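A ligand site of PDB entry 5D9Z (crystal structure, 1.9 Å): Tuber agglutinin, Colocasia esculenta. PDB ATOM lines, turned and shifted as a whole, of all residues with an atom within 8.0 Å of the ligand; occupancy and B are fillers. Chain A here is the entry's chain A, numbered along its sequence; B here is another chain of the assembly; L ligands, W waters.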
ATOM      1  N   LEU A  33      21.789  24.593  25.604  1.00  0.00           N
ATOM      2  CA  LEU A  33      22.775  23.530  25.462  1.00  0.00           C
ATOM      3  C   LEU A  33      22.548  22.856  24.135  1.00  0.00           C
ATOM      4  O   LEU A  33      21.559  22.163  23.937  1.00  0.00           O
ATOM      5  CB  LEU A  33      22.656  22.494  26.571  1.00  0.00           C
ATOM      6  CG  LEU A  33      23.861  21.589  26.730  1.00  0.00           C
ATOM      7  CD1 LEU A  33      25.119  22.414  26.748  1.00  0.00           C
ATOM      8  CD2 LEU A  33      23.749  20.812  28.013  1.00  0.00           C
ATOM      9  N   TRP A  40      20.393  17.641  18.845  1.00  0.00           N
ATOM     10  CA  TRP A  40      19.806  17.651  20.158  1.00  0.00           C
ATOM     11  C   TRP A  40      20.072  18.969  20.825  1.00  0.00           C
ATOM     12  O   TRP A  40      21.129  19.579  20.626  1.00  0.00           O
ATOM     13  CB  TRP A  40      20.354  16.502  21.014  1.00  0.00           C
ATOM     14  CG  TRP A  40      19.758  16.505  22.369  1.00  0.00           C
ATOM     15  CD1 TRP A  40      18.696  15.771  22.803  1.00  0.00           C
ATOM     16  CD2 TRP A  40      20.181  17.306  23.479  1.00  0.00           C
ATOM     17  NE1 TRP A  40      18.443  16.057  24.121  1.00  0.00           N
ATOM     18  CE2 TRP A  40      19.343  17.002  24.556  1.00  0.00           C
ATOM     19  CE3 TRP A  40      21.217  18.223  23.664  1.00  0.00           C
ATOM     20  CZ2 TRP A  40      19.481  17.595  25.801  1.00  0.00           C
ATOM     21  CZ3 TRP A  40      21.350  18.832  24.894  1.00  0.00           C
ATOM     22  CH2 TRP A  40      20.487  18.512  25.956  1.00  0.00           C
ATOM     23  N   GLN A  41      19.114  19.427  21.619  1.00  0.00           N
ATOM     24  CA  GLN A  41      19.363  20.593  22.439  1.00  0.00           C
ATOM     25  C   GLN A  41      18.583  20.501  23.728  1.00  0.00           C
ATOM     26  O   GLN A  41      17.588  19.791  23.818  1.00  0.00           O
ATOM     27  CB  GLN A  41      18.972  21.843  21.701  1.00  0.00           C
ATOM     28  CG  GLN A  41      17.554  21.791  21.256  1.00  0.00           C
ATOM     29  CD  GLN A  41      17.155  23.053  20.532  1.00  0.00           C
ATOM     30  OE1 GLN A  41      17.486  24.151  20.965  1.00  0.00           O
ATOM     31  NE2 GLN A  41      16.463  22.892  19.417  1.00  0.00           N
ATOM     32  N   SER A  42      19.072  21.208  24.741  1.00  0.00           N
ATOM     33  CA  SER A  42      18.303  21.365  25.947  1.00  0.00           C
ATOM     34  C   SER A  42      17.040  22.073  25.524  1.00  0.00           C
ATOM     35  O   SER A  42      15.972  21.822  26.058  1.00  0.00           O
ATOM     36  CB  SER A  42      19.056  22.240  26.943  1.00  0.00           C
ATOM     37  OG  SER A  42      19.402  23.472  26.344  1.00  0.00           O
ATOM     38  N   ASN A  43      17.199  22.962  24.540  1.00  0.00           N
ATOM     39  CA  ASN A  43      16.110  23.771  24.020  1.00  0.00           C
ATOM     40  C   ASN A  43      15.632  24.758  25.073  1.00  0.00           C
ATOM     41  O   ASN A  43      14.490  24.756  25.492  1.00  0.00           O
ATOM     42  CB  ASN A  43      14.972  22.888  23.516  1.00  0.00           C
ATOM     43  CG  ASN A  43      13.843  23.680  22.919  1.00  0.00           C
ATOM     44  OD1 ASN A  43      14.009  24.845  22.540  1.00  0.00           O
ATOM     45  ND2 ASN A  43      12.675  23.064  22.825  1.00  0.00           N
ATOM     46  N   THR A  44      16.554  25.607  25.500  1.00  0.00           N
ATOM     47  CA  THR A  44      16.305  26.550  26.573  1.00  0.00           C
ATOM     48  C   THR A  44      16.959  27.874  26.266  1.00  0.00           C
ATOM     49  O   THR A  44      17.537  28.501  27.155  1.00  0.00           O
ATOM     50  CB  THR A  44      16.923  26.066  27.870  1.00  0.00           C
ATOM     51  OG1 THR A  44      18.311  25.795  27.650  1.00  0.00           O
ATOM     52  CG2 THR A  44      16.249  24.819  28.342  1.00  0.00           C
ATOM     53  N   GLU A  60      21.733  13.171  37.473  1.00  0.00           N
ATOM     54  CA  GLU A  60      20.825  14.021  36.714  1.00  0.00           C
ATOM     55  C   GLU A  60      21.588  15.242  36.200  1.00  0.00           C
ATOM     56  O   GLU A  60      22.402  15.817  36.912  1.00  0.00           O
ATOM     57  CB  GLU A  60      19.627  14.445  37.570  1.00  0.00           C
ATOM     58  CG  GLU A  60      18.705  15.457  36.883  1.00  0.00           C
ATOM     59  CD  GLU A  60      17.411  15.706  37.644  1.00  0.00           C
ATOM     60  OE1 GLU A  60      17.427  15.671  38.892  1.00  0.00           O
ATOM     61  OE2 GLU A  60      16.375  15.936  36.990  1.00  0.00           O
ATOM     62  N   LEU A  61      21.345  15.628  34.951  1.00  0.00           N
ATOM     63  CA  LEU A  61      21.967  16.814  34.387  1.00  0.00           C
ATOM     64  C   LEU A  61      21.023  18.006  34.630  1.00  0.00           C
ATOM     65  O   LEU A  61      19.823  17.937  34.333  1.00  0.00           O
ATOM     66  CB  LEU A  61      22.261  16.628  32.902  1.00  0.00           C
ATOM     67  CG  LEU A  61      23.301  15.555  32.560  1.00  0.00           C
ATOM     68  CD1 LEU A  61      23.047  15.044  31.172  1.00  0.00           C
ATOM     69  CD2 LEU A  61      24.691  16.132  32.640  1.00  0.00           C
ATOM     70  N   VAL A  71      16.758  25.271  35.012  1.00  0.00           N
ATOM     71  CA  VAL A  71      16.118  25.662  33.751  1.00  0.00           C
ATOM     72  C   VAL A  71      15.824  24.436  32.897  1.00  0.00           C
ATOM     73  O   VAL A  71      14.964  24.466  32.026  1.00  0.00           O
ATOM     74  CB  VAL A  71      17.015  26.602  32.936  1.00  0.00           C
ATOM     75  CG1 VAL A  71      16.215  27.327  31.862  1.00  0.00           C
ATOM     76  CG2 VAL A  71      17.690  27.599  33.846  1.00  0.00           C
ATOM     77  N   TRP A  72      16.573  23.363  33.148  1.00  0.00           N
ATOM     78  CA  TRP A  72      16.310  22.077  32.513  1.00  0.00           C
ATOM     79  C   TRP A  72      16.875  20.981  33.419  1.00  0.00           C
ATOM     80  O   TRP A  72      17.929  21.142  34.022  1.00  0.00           O
ATOM     81  CB  TRP A  72      16.920  22.048  31.088  1.00  0.00           C
ATOM     82  CG  TRP A  72      16.823  20.729  30.279  1.00  0.00           C
ATOM     83  CD1 TRP A  72      15.879  20.381  29.342  1.00  0.00           C
ATOM     84  CD2 TRP A  72      17.754  19.642  30.320  1.00  0.00           C
ATOM     85  NE1 TRP A  72      16.160  19.134  28.821  1.00  0.00           N
ATOM     86  CE2 TRP A  72      17.303  18.661  29.407  1.00  0.00           C
ATOM     87  CE3 TRP A  72      18.923  19.393  31.049  1.00  0.00           C
ATOM     88  CZ2 TRP A  72      17.992  17.465  29.209  1.00  0.00           C
ATOM     89  CZ3 TRP A  72      19.596  18.215  30.855  1.00  0.00           C
ATOM     90  CH2 TRP A  72      19.132  17.261  29.941  1.00  0.00           C
ATOM     91  N   ARG A  73      16.137  19.889  33.565  1.00  0.00           N
ATOM     92  CA  ARG A  73      16.617  18.744  34.310  1.00  0.00           C
ATOM     93  C   ARG A  73      16.569  17.633  33.278  1.00  0.00           C
ATOM     94  O   ARG A  73      15.836  17.752  32.294  1.00  0.00           O
ATOM     95  CB  ARG A  73      15.701  18.459  35.497  1.00  0.00           C
ATOM     96  CG  ARG A  73      15.884  19.429  36.661  1.00  0.00           C
ATOM     97  CD  ARG A  73      14.711  19.451  37.642  1.00  0.00           C
ATOM     98  NE  ARG A  73      14.783  18.403  38.658  1.00  0.00           N
ATOM     99  CZ  ARG A  73      15.469  18.495  39.796  1.00  0.00           C
ATOM    100  NH1 ARG A  73      16.155  19.597  40.073  1.00  0.00           N
ATOM    101  NH2 ARG A  73      15.469  17.485  40.657  1.00  0.00           N
ATOM    102  N   SER A  74      17.362  16.585  33.436  1.00  0.00           N
ATOM    103  CA  SER A  74      17.290  15.457  32.500  1.00  0.00           C
ATOM    104  C   SER A  74      16.179  14.523  32.929  1.00  0.00           C
ATOM    105  O   SER A  74      15.768  13.635  32.172  1.00  0.00           O
ATOM    106  CB  SER A  74      18.617  14.701  32.412  1.00  0.00           C
ATOM    107  OG  SER A  74      19.102  14.345  33.686  1.00  0.00           O
ATOM    108  N   ARG A  75      15.725  14.733  34.168  1.00  0.00           N
ATOM    109  CA  ARG A  75      14.611  14.006  34.778  1.00  0.00           C
ATOM    110  C   ARG A  75      14.918  12.543  35.125  1.00  0.00           C
ATOM    111  O   ARG A  75      14.128  11.882  35.791  1.00  0.00           O
ATOM    112  CB  ARG A  75      13.333  14.153  33.945  1.00  0.00           C
ATOM    113  CG  ARG A  75      13.027  15.596  33.531  1.00  0.00           C
ATOM    114  CD  ARG A  75      11.542  15.881  33.421  1.00  0.00           C
ATOM    115  NE  ARG A  75      11.285  17.312  33.544  1.00  0.00           N
ATOM    116  CZ  ARG A  75      11.153  18.151  32.523  1.00  0.00           C
ATOM    117  NH1 ARG A  75      11.246  17.712  31.283  1.00  0.00           N
ATOM    118  NH2 ARG A  75      10.915  19.436  32.746  1.00  0.00           N
ATOM    119  N   ALA A  76      16.063  12.030  34.687  1.00  0.00           N
ATOM    120  CA  ALA A  76      16.428  10.637  34.997  1.00  0.00           C
ATOM    121  C   ALA A  76      17.026  10.518  36.394  1.00  0.00           C
ATOM    122  O   ALA A  76      17.848  11.342  36.800  1.00  0.00           O
ATOM    123  CB  ALA A  76      17.383  10.075  33.951  1.00  0.00           C
ATOM    124  N   TRP B 106      20.412   7.717  31.175  1.00  0.00           N
ATOM    125  CA  TRP B 106      19.823   8.780  30.393  1.00  0.00           C
ATOM    126  C   TRP B 106      20.628   9.090  29.111  1.00  0.00           C
ATOM    127  O   TRP B 106      21.855   9.083  29.136  1.00  0.00           O
ATOM    128  CB  TRP B 106      19.693  10.034  31.242  1.00  0.00           C
ATOM    129  CG  TRP B 106      19.038  11.104  30.502  1.00  0.00           C
ATOM    130  CD1 TRP B 106      17.716  11.311  30.391  1.00  0.00           C
ATOM    131  CD2 TRP B 106      19.680  12.089  29.678  1.00  0.00           C
ATOM    132  NE1 TRP B 106      17.481  12.392  29.567  1.00  0.00           N
ATOM    133  CE2 TRP B 106      18.669  12.886  29.114  1.00  0.00           C
ATOM    134  CE3 TRP B 106      21.004  12.376  29.369  1.00  0.00           C
ATOM    135  CZ2 TRP B 106      18.951  13.955  28.262  1.00  0.00           C
ATOM    136  CZ3 TRP B 106      21.283  13.436  28.522  1.00  0.00           C
ATOM    137  CH2 TRP B 106      20.253  14.214  27.977  1.00  0.00           C
ATOM    138  N   GLU B 107      19.927   9.372  28.014  1.00  0.00           N
ATOM    139  CA  GLU B 107      20.594   9.685  26.739  1.00  0.00           C
ATOM    140  C   GLU B 107      19.886  10.779  25.923  1.00  0.00           C
ATOM    141  O   GLU B 107      18.688  11.035  26.119  1.00  0.00           O
ATOM    142  CB  GLU B 107      20.735   8.417  25.893  1.00  0.00           C
ATOM    143  CG  GLU B 107      19.392   7.908  25.340  1.00  0.00           C
ATOM    144  CD  GLU B 107      19.461   6.506  24.728  1.00  0.00           C
ATOM    145  OE1 GLU B 107      18.432   6.039  24.189  1.00  0.00           O
ATOM    146  OE2 GLU B 107      20.542   5.883  24.803  1.00  0.00           O
ATOM    147  N   THR B 108      20.606  11.419  25.014  1.00  0.00           N
ATOM    148  CA  THR B 108      20.003  12.394  24.114  1.00  0.00           C
ATOM    149  C   THR B 108      19.190  11.705  23.006  1.00  0.00           C
ATOM    150  O   THR B 108      18.285  12.311  22.416  1.00  0.00           O
ATOM    151  CB  THR B 108      21.073  13.293  23.524  1.00  0.00           C
ATOM    152  OG1 THR B 108      22.238  12.514  23.267  1.00  0.00           O
ATOM    153  CG2 THR B 108      21.430  14.375  24.499  1.00  0.00           C
ATOM    154  N   SER B 109      19.518  10.439  22.735  1.00  0.00           N
ATOM    155  CA  SER B 109      18.862   9.641  21.689  1.00  0.00           C
ATOM    156  C   SER B 109      19.406   8.200  21.732  1.00  0.00           C
ATOM    157  O   SER B 109      20.445   7.974  22.356  1.00  0.00           O
ATOM    158  CB  SER B 109      19.119  10.275  20.336  1.00  0.00           C
ATOM    159  OG  SER B 109      20.377  10.919  20.359  1.00  0.00           O
HETATM  160  C1  LIG L   1      13.290  15.970  25.957  1.00  0.00           C
HETATM  161  C2  LIG L   1      14.682  16.498  25.631  1.00  0.00           C
HETATM  162  C3  LIG L   1      15.640  15.609  26.407  1.00  0.00           C
HETATM  163  C4  LIG L   1      15.320  15.647  27.899  1.00  0.00           C
HETATM  164  C5  LIG L   1      13.849  15.442  28.202  1.00  0.00           C
HETATM  165  C6  LIG L   1      13.558  15.880  29.642  1.00  0.00           C
HETATM  166  O1  LIG L   1      12.337  16.620  25.137  1.00  0.00           O
HETATM  167  O2  LIG L   1      14.872  17.856  26.016  1.00  0.00           O
HETATM  168  O3  LIG L   1      16.920  16.121  26.199  1.00  0.00           O
HETATM  169  O4  LIG L   1      16.016  14.604  28.528  1.00  0.00           O
HETATM  170  O5  LIG L   1      13.025  16.197  27.329  1.00  0.00           O
HETATM  171  O6  LIG L   1      13.686  17.281  29.736  1.00  0.00           O
HETATM  172  O   HOH W   1      11.544  18.511  28.567  1.00  0.00           O
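Residues that only touch the ligand: Gln 41 (3.99 Å) and Ser 74 (3.8 Å).
Seven residues have an atom within 4 Å of the ligand: Trp 40, Gln 41, Trp 72, Arg 73, Ser 74, Arg 75 and Trp 106 of chain B.
Water W1 lies within hydrogen-bond range of an oxygen (O6) of the ligand (2.7 Å) and the guanidinium group (NH1) of Arg 75 (2.8 Å).
The guanidinium group of Arg 73 is in salt-bridge range of the side-chain carboxylate of Glu 60 (3.2 Å).
OG of Ser 74 is in hydrogen-bond range of N of Leu 61, 2.9 Å away.
The backbone NH (N) of Arg 75 is in hydrogen-bond range of the side-chain carboxylate (OE2) of Glu 60 (3.1 Å).
NE1 of Trp 106 of chain B lies within hydrogen-bond range of O of Ser 74 (3.4 Å).
O3 of the ligand lies within hydrogen-bond range of NE1 of Trp 40 (2.6 Å).
The indole nitrogen (NE1) of Trp 72 lies within hydrogen-bond range of an oxygen (O6) of the ligand (3.2 Å).
NE1 of Trp 106 of chain B sits at hydrogen-bond distance from O4 of the ligand (2.8 Å).
The guanidinium group (NH1) of Arg 75 is in hydrogen-bond range of an oxygen (O6) of the ligand, at 2.9 Å.
An oxygen (O6) of the ligand sits at hydrogen-bond distance from the backbone carbonyl oxygen of Arg 73.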
